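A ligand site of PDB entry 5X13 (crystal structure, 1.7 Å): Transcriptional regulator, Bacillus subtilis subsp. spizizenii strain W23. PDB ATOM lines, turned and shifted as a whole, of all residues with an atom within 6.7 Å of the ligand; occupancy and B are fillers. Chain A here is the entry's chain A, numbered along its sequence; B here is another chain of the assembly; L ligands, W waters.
An oxygen (O2) of the ligand sits at hydrogen-bond distance from the side-chain hydroxyl (OG1) of Thr 99 of chain B (2.6 Å).
The side-chain amino group of Lys 133 is in salt-bridge range of an oxygen (O2) of the ligand.
A ring nitrogen (NE2) of His 160 lies within hydrogen-bond range of an oxygen (O3) of the ligand, 2.8 Å away.
NH2 of Arg 170 is in salt-bridge range of O2 of the ligand (2.9 Å).
The backbone carbonyl oxygen of Asp 136 lies within hydrogen-bond range of the side-chain hydroxyl of Ser 140 (3.4 Å).
NH2 of Arg 170 is in hydrogen-bond range of OG1 of Thr 99 of chain B (3.5 Å).
OE2 of Glu 171 lies within salt-bridge range of NH2 of Arg 170 (3.0 Å).
OH of Tyr 109 of chain B is in hydrogen-bond range of OE2 of Glu 35.
A ring nitrogen (ND1) of His 160 sits at hydrogen-bond distance from the side-chain carboxylate (OE2) of Glu 35 (3.5 Å).
Merely in contact with the ligand: Glu 35 (3.4 Å), Gln 38 (3.6 Å), Phe 39 (3.6 Å), Leu 137 (3.7 Å), Ser 140 (3.8 Å), Val 163 (3.97 Å), Leu 164 (3.9 Å) and Ala 167 (3.5 Å).
Water W1 bridges O of Val 163 (2.9 Å) and O1 of the ligand (2.9 Å).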
ATOM      1  N   GLU A  34      22.508  10.865  13.130  1.00  0.00           N
ATOM      2  CA  GLU A  34      23.506  10.031  13.836  1.00  0.00           C
ATOM      3  C   GLU A  34      23.614   8.715  13.065  1.00  0.00           C
ATOM      4  O   GLU A  34      23.681   8.715  11.837  1.00  0.00           O
ATOM      5  CB  GLU A  34      23.117   9.738  15.307  1.00  0.00           C
ATOM      6  CG  GLU A  34      22.825  10.927  16.257  1.00  0.00           C
ATOM      7  CD  GLU A  34      21.851  10.507  17.392  1.00  0.00           C
ATOM      8  N   GLU A  35      23.567   7.589  13.780  1.00  0.00           N
ATOM      9  CA  GLU A  35      23.977   6.327  13.195  1.00  0.00           C
ATOM     10  C   GLU A  35      23.056   5.858  12.126  1.00  0.00           C
ATOM     11  O   GLU A  35      23.482   5.296  11.147  1.00  0.00           O
ATOM     12  CB  GLU A  35      24.229   5.233  14.290  1.00  0.00           C
ATOM     13  CG  GLU A  35      22.994   4.651  14.976  1.00  0.00           C
ATOM     14  CD  GLU A  35      22.694   5.164  16.425  1.00  0.00           C
ATOM     15  OE1 GLU A  35      23.299   6.152  16.909  1.00  0.00           O
ATOM     16  OE2 GLU A  35      21.856   4.523  17.104  1.00  0.00           O
ATOM     17  N   LEU A  36      21.760   6.147  12.290  1.00  0.00           N
ATOM     18  CA  LEU A  36      20.777   5.678  11.377  1.00  0.00           C
ATOM     19  C   LEU A  36      21.018   6.202   9.977  1.00  0.00           C
ATOM     20  O   LEU A  36      20.855   5.462   9.019  1.00  0.00           O
ATOM     21  CB  LEU A  36      19.375   6.041  11.899  1.00  0.00           C
ATOM     22  CG  LEU A  36      18.149   5.518  11.235  1.00  0.00           C
ATOM     23  CD1 LEU A  36      18.144   3.970  11.037  1.00  0.00           C
ATOM     24  CD2 LEU A  36      16.892   6.010  12.006  1.00  0.00           C
ATOM     25  N   GLN A  38      23.830   6.697   8.636  1.00  0.00           N
ATOM     26  CA  GLN A  38      24.975   6.040   8.042  1.00  0.00           C
ATOM     27  C   GLN A  38      24.587   4.793   7.241  1.00  0.00           C
ATOM     28  O   GLN A  38      25.252   4.448   6.288  1.00  0.00           O
ATOM     29  CB  GLN A  38      25.982   5.689   9.140  1.00  0.00           C
ATOM     30  CG  GLN A  38      26.532   6.944   9.798  1.00  0.00           C
ATOM     31  CD  GLN A  38      27.375   7.732   8.858  1.00  0.00           C
ATOM     32  OE1 GLN A  38      28.379   7.234   8.344  1.00  0.00           O
ATOM     33  NE2 GLN A  38      27.006   9.005   8.659  1.00  0.00           N
ATOM     34  N   PHE A  39      23.545   4.112   7.631  1.00  0.00           N
ATOM     35  CA  PHE A  39      23.105   2.895   6.921  1.00  0.00           C
ATOM     36  C   PHE A  39      21.652   2.936   6.402  1.00  0.00           C
ATOM     37  O   PHE A  39      21.235   2.006   5.690  1.00  0.00           O
ATOM     38  CB  PHE A  39      23.329   1.688   7.830  1.00  0.00           C
ATOM     39  CG  PHE A  39      22.418   1.673   9.047  1.00  0.00           C
ATOM     40  CD1 PHE A  39      22.812   2.324  10.229  1.00  0.00           C
ATOM     41  CD2 PHE A  39      21.209   0.993   9.054  1.00  0.00           C
ATOM     42  CE1 PHE A  39      21.961   2.311  11.361  1.00  0.00           C
ATOM     43  CE2 PHE A  39      20.381   0.971  10.205  1.00  0.00           C
ATOM     44  CZ  PHE A  39      20.787   1.665  11.357  1.00  0.00           C
ATOM     45  N   LYS A 133      37.482   4.676   5.768  1.00  0.00           N
ATOM     46  CA  LYS A 133      36.124   4.400   6.214  1.00  0.00           C
ATOM     47  C   LYS A 133      36.106   3.420   7.390  1.00  0.00           C
ATOM     48  O   LYS A 133      35.378   3.595   8.378  1.00  0.00           O
ATOM     49  CB  LYS A 133      35.288   3.856   5.100  1.00  0.00           C
ATOM     50  CG  LYS A 133      33.845   3.574   5.489  1.00  0.00           C
ATOM     51  CD  LYS A 133      33.018   3.187   4.296  1.00  0.00           C
ATOM     52  CE  LYS A 133      31.564   2.937   4.699  1.00  0.00           C
ATOM     53  NZ  LYS A 133      30.917   4.259   5.014  1.00  0.00           N
ATOM     54  N   ASP A 136      36.986   5.183  10.583  1.00  0.00           N
ATOM     55  CA  ASP A 136      35.840   5.906  11.085  1.00  0.00           C
ATOM     56  C   ASP A 136      34.832   4.982  11.796  1.00  0.00           C
ATOM     57  O   ASP A 136      34.313   5.324  12.877  1.00  0.00           O
ATOM     58  CB  ASP A 136      35.085   6.601   9.955  1.00  0.00           C
ATOM     59  CG  ASP A 136      35.884   7.712   9.265  1.00  0.00           C
ATOM     60  OD1 ASP A 136      36.911   8.155   9.819  1.00  0.00           O
ATOM     61  OD2 ASP A 136      35.442   8.129   8.154  1.00  0.00           O
ATOM     62  N   LEU A 137      34.570   3.825  11.182  1.00  0.00           N
ATOM     63  CA  LEU A 137      33.646   2.859  11.802  1.00  0.00           C
ATOM     64  C   LEU A 137      34.197   2.319  13.121  1.00  0.00           C
ATOM     65  O   LEU A 137      33.462   2.152  14.107  1.00  0.00           O
ATOM     66  CB  LEU A 137      33.362   1.712  10.865  1.00  0.00           C
ATOM     67  CG  LEU A 137      32.571   2.058   9.615  1.00  0.00           C
ATOM     68  CD1 LEU A 137      32.619   0.879   8.646  1.00  0.00           C
ATOM     69  CD2 LEU A 137      31.117   2.432   9.988  1.00  0.00           C
ATOM     70  N   SER A 140      33.420   4.836  15.740  1.00  0.00           N
ATOM     71  CA  SER A 140      32.054   4.721  16.180  1.00  0.00           C
ATOM     72  C   SER A 140      31.837   3.516  17.090  1.00  0.00           C
ATOM     73  O   SER A 140      31.049   3.587  18.038  1.00  0.00           O
ATOM     74  CB  SER A 140      31.134   4.611  14.968  1.00  0.00           C
ATOM     75  OG  SER A 140      31.244   5.754  14.161  1.00  0.00           O
ATOM     76  N   TYR A 141      32.539   2.432  16.772  1.00  0.00           N
ATOM     77  CA  TYR A 141      32.473   1.178  17.552  1.00  0.00           C
ATOM     78  C   TYR A 141      33.034   1.382  18.952  1.00  0.00           C
ATOM     79  O   TYR A 141      32.435   1.025  19.958  1.00  0.00           O
ATOM     80  CB  TYR A 141      33.182   0.079  16.771  1.00  0.00           C
ATOM     81  CG  TYR A 141      33.171  -1.235  17.481  1.00  0.00           C
ATOM     82  CD1 TYR A 141      32.001  -1.985  17.603  1.00  0.00           C
ATOM     83  CD2 TYR A 141      34.332  -1.715  18.059  1.00  0.00           C
ATOM     84  CE1 TYR A 141      32.024  -3.185  18.316  1.00  0.00           C
ATOM     85  CE2 TYR A 141      34.353  -2.907  18.744  1.00  0.00           C
ATOM     86  CZ  TYR A 141      33.208  -3.621  18.874  1.00  0.00           C
ATOM     87  OH  TYR A 141      33.273  -4.801  19.593  1.00  0.00           O
ATOM     88  N   LEU A 144      30.564   3.405  21.024  1.00  0.00           N
ATOM     89  CA  LEU A 144      29.476   2.538  21.446  1.00  0.00           C
ATOM     90  C   LEU A 144      29.926   1.697  22.626  1.00  0.00           C
ATOM     91  O   LEU A 144      29.201   1.591  23.630  1.00  0.00           O
ATOM     92  CB  LEU A 144      29.010   1.649  20.292  1.00  0.00           C
ATOM     93  CG  LEU A 144      27.959   0.581  20.691  1.00  0.00           C
ATOM     94  CD1 LEU A 144      26.761   1.296  21.283  1.00  0.00           C
ATOM     95  CD2 LEU A 144      27.499  -0.306  19.531  1.00  0.00           C
ATOM     96  N   HIS A 160      22.215  -1.473  17.889  1.00  0.00           N
ATOM     97  CA  HIS A 160      23.259  -0.572  17.423  1.00  0.00           C
ATOM     98  C   HIS A 160      24.553  -1.381  17.181  1.00  0.00           C
ATOM     99  O   HIS A 160      25.244  -1.204  16.185  1.00  0.00           O
ATOM    100  CB  HIS A 160      23.480   0.528  18.440  1.00  0.00           C
ATOM    101  CG  HIS A 160      24.288   1.643  17.935  1.00  0.00           C
ATOM    102  ND1 HIS A 160      24.446   2.813  18.654  1.00  0.00           N
ATOM    103  CD2 HIS A 160      25.029   1.786  16.802  1.00  0.00           C
ATOM    104  CE1 HIS A 160      25.215   3.642  17.961  1.00  0.00           C
ATOM    105  NE2 HIS A 160      25.590   3.052  16.850  1.00  0.00           N
ATOM    106  N   VAL A 163      24.333  -3.319  13.819  1.00  0.00           N
ATOM    107  CA  VAL A 163      24.550  -2.562  12.570  1.00  0.00           C
ATOM    108  C   VAL A 163      26.039  -2.132  12.470  1.00  0.00           C
ATOM    109  O   VAL A 163      26.562  -2.131  11.373  1.00  0.00           O
ATOM    110  CB  VAL A 163      23.582  -1.359  12.406  1.00  0.00           C
ATOM    111  CG1 VAL A 163      22.194  -1.873  12.254  1.00  0.00           C
ATOM    112  CG2 VAL A 163      23.630  -0.406  13.606  1.00  0.00           C
ATOM    113  N   LEU A 164      26.662  -1.816  13.595  1.00  0.00           N
ATOM    114  CA  LEU A 164      28.037  -1.388  13.571  1.00  0.00           C
ATOM    115  C   LEU A 164      29.005  -2.537  13.303  1.00  0.00           C
ATOM    116  O   LEU A 164      29.914  -2.375  12.488  1.00  0.00           O
ATOM    117  CB  LEU A 164      28.427  -0.656  14.838  1.00  0.00           C
ATOM    118  CG  LEU A 164      29.785   0.035  14.778  1.00  0.00           C
ATOM    119  CD1 LEU A 164      30.041   0.858  13.489  1.00  0.00           C
ATOM    120  CD2 LEU A 164      29.807   0.931  15.945  1.00  0.00           C
ATOM    121  N   THR A 165      28.805  -3.687  13.931  1.00  0.00           N
ATOM    122  CA  THR A 165      29.678  -4.835  13.672  1.00  0.00           C
ATOM    123  C   THR A 165      29.508  -5.289  12.231  1.00  0.00           C
ATOM    124  O   THR A 165      30.485  -5.756  11.599  1.00  0.00           O
ATOM    125  CB  THR A 165      29.497  -5.955  14.678  1.00  0.00           C
ATOM    126  OG1 THR A 165      28.137  -6.420  14.674  1.00  0.00           O
ATOM    127  CG2 THR A 165      29.862  -5.517  16.117  1.00  0.00           C
ATOM    128  N   LYS A 166      28.282  -5.262  11.727  1.00  0.00           N
ATOM    129  CA  LYS A 166      28.044  -5.616  10.358  1.00  0.00           C
ATOM    130  C   LYS A 166      28.909  -4.741   9.429  1.00  0.00           C
ATOM    131  O   LYS A 166      29.561  -5.245   8.491  1.00  0.00           O
ATOM    132  CB  LYS A 166      26.570  -5.459   9.992  1.00  0.00           C
ATOM    133  CG  LYS A 166      26.260  -5.784   8.547  1.00  0.00           C
ATOM    134  CD  LYS A 166      26.347  -7.290   8.353  1.00  0.00           C
ATOM    135  CE  LYS A 166      25.994  -7.676   6.960  1.00  0.00           C
ATOM    136  NZ  LYS A 166      27.179  -7.717   6.096  1.00  0.00           N
ATOM    137  N   ALA A 167      28.864  -3.433   9.664  1.00  0.00           N
ATOM    138  CA  ALA A 167      29.586  -2.461   8.847  1.00  0.00           C
ATOM    139  C   ALA A 167      31.102  -2.635   8.914  1.00  0.00           C
ATOM    140  O   ALA A 167      31.780  -2.644   7.881  1.00  0.00           O
ATOM    141  CB  ALA A 167      29.214  -1.062   9.243  1.00  0.00           C
ATOM    142  N   LEU A 168      31.585  -2.876  10.117  1.00  0.00           N
ATOM    143  CA  LEU A 168      33.004  -3.130  10.379  1.00  0.00           C
ATOM    144  C   LEU A 168      33.479  -4.367   9.621  1.00  0.00           C
ATOM    145  O   LEU A 168      34.451  -4.302   8.875  1.00  0.00           O
ATOM    146  CB  LEU A 168      33.263  -3.341  11.865  1.00  0.00           C
ATOM    147  CG  LEU A 168      33.257  -2.149  12.722  1.00  0.00           C
ATOM    148  CD1 LEU A 168      33.135  -2.620  14.186  1.00  0.00           C
ATOM    149  CD2 LEU A 168      34.567  -1.294  12.457  1.00  0.00           C
ATOM    150  N   ARG A 170      31.994  -5.803   7.055  1.00  0.00           N
ATOM    151  CA  ARG A 170      31.826  -5.562   5.626  1.00  0.00           C
ATOM    152  C   ARG A 170      33.042  -4.823   5.052  1.00  0.00           C
ATOM    153  O   ARG A 170      33.612  -5.205   4.020  1.00  0.00           O
ATOM    154  CB  ARG A 170      30.590  -4.700   5.392  1.00  0.00           C
ATOM    155  CG  ARG A 170      30.301  -4.376   3.961  1.00  0.00           C
ATOM    156  CD  ARG A 170      29.051  -3.372   3.838  1.00  0.00           C
ATOM    157  NE  ARG A 170      29.532  -2.070   4.286  1.00  0.00           N
ATOM    158  CZ  ARG A 170      28.941  -1.237   5.129  1.00  0.00           C
ATOM    159  NH1 ARG A 170      27.751  -1.467   5.642  1.00  0.00           N
ATOM    160  NH2 ARG A 170      29.559  -0.107   5.445  1.00  0.00           N
ATOM    161  N   GLU A 171      33.434  -3.758   5.730  1.00  0.00           N
ATOM    162  CA  GLU A 171      34.554  -2.958   5.243  1.00  0.00           C
ATOM    163  C   GLU A 171      35.890  -3.655   5.448  1.00  0.00           C
ATOM    164  O   GLU A 171      36.746  -3.594   4.587  1.00  0.00           O
ATOM    165  CB  GLU A 171      34.571  -1.564   5.862  1.00  0.00           C
ATOM    166  CG  GLU A 171      33.382  -0.702   5.515  1.00  0.00           C
ATOM    167  CD  GLU A 171      33.103  -0.540   4.020  1.00  0.00           C
ATOM    168  OE1 GLU A 171      34.062  -0.562   3.186  1.00  0.00           O
ATOM    169  OE2 GLU A 171      31.912  -0.390   3.683  1.00  0.00           O
ATOM    170  N   GLU B  98      27.540   6.230  -0.416  1.00  0.00           N
ATOM    171  CA  GLU B  98      26.724   6.009   0.775  1.00  0.00           C
ATOM    172  C   GLU B  98      26.325   4.552   0.859  1.00  0.00           C
ATOM    173  O   GLU B  98      26.169   3.835  -0.170  1.00  0.00           O
ATOM    174  CB  GLU B  98      25.476   6.930   0.784  1.00  0.00           C
ATOM    175  N   THR B  99      26.204   4.077   2.077  1.00  0.00           N
ATOM    176  CA  THR B  99      25.891   2.673   2.295  1.00  0.00           C
ATOM    177  C   THR B  99      24.530   2.349   1.775  1.00  0.00           C
ATOM    178  O   THR B  99      23.564   3.095   1.997  1.00  0.00           O
ATOM    179  CB  THR B  99      26.031   2.292   3.789  1.00  0.00           C
ATOM    180  OG1 THR B  99      27.415   2.290   4.110  1.00  0.00           O
ATOM    181  CG2 THR B  99      25.469   0.901   4.130  1.00  0.00           C
ATOM    182  N   VAL B 100      24.493   1.198   1.095  1.00  0.00           N
ATOM    183  CA  VAL B 100      23.320   0.683   0.428  1.00  0.00           C
ATOM    184  C   VAL B 100      22.354   0.189   1.501  1.00  0.00           C
ATOM    185  O   VAL B 100      22.781  -0.478   2.432  1.00  0.00           O
ATOM    186  CB  VAL B 100      23.732  -0.475  -0.552  1.00  0.00           C
ATOM    187  N   TYR B 109      18.661  -3.580  13.656  1.00  0.00           N
ATOM    188  CA  TYR B 109      18.770  -2.373  14.472  1.00  0.00           C
ATOM    189  C   TYR B 109      17.651  -2.312  15.525  1.00  0.00           C
ATOM    190  O   TYR B 109      17.835  -1.814  16.632  1.00  0.00           O
ATOM    191  CB  TYR B 109      18.763  -1.162  13.574  1.00  0.00           C
ATOM    192  CG  TYR B 109      19.009   0.167  14.207  1.00  0.00           C
ATOM    193  CD1 TYR B 109      20.217   0.465  14.857  1.00  0.00           C
ATOM    194  CD2 TYR B 109      18.079   1.177  14.097  1.00  0.00           C
ATOM    195  CE1 TYR B 109      20.429   1.695  15.376  1.00  0.00           C
ATOM    196  CE2 TYR B 109      18.284   2.397  14.635  1.00  0.00           C
ATOM    197  CZ  TYR B 109      19.484   2.671  15.268  1.00  0.00           C
ATOM    198  OH  TYR B 109      19.775   3.909  15.809  1.00  0.00           O
HETATM  199  C1  LIG L   1      27.453   1.648   7.515  1.00  0.00           C
HETATM  200  O1  LIG L   1      26.692   0.616   7.400  1.00  0.00           O
HETATM  201  O2  LIG L   1      28.129   2.097   6.576  1.00  0.00           O
HETATM  202  C2  LIG L   1      27.595   2.320   8.791  1.00  0.00           C
HETATM  203  C3  LIG L   1      26.922   1.980   9.862  1.00  0.00           C
HETATM  204  C4  LIG L   1      27.097   2.646  11.167  1.00  0.00           C
HETATM  205  C5  LIG L   1      26.348   2.130  12.199  1.00  0.00           C
HETATM  206  C6  LIG L   1      26.456   2.614  13.487  1.00  0.00           C
HETATM  207  C7  LIG L   1      27.350   3.676  13.746  1.00  0.00           C
HETATM  208  C8  LIG L   1      28.081   4.216  12.706  1.00  0.00           C
HETATM  209  C9  LIG L   1      27.995   3.694  11.425  1.00  0.00           C
HETATM  210  O3  LIG L   1      27.399   4.143  15.014  1.00  0.00           O
HETATM  211  O   HOH W   1      25.249  -1.507   8.852  1.00  0.00           O
HETATM  212  O   HOH W   2      27.855   6.652  15.737  1.00  0.00           O
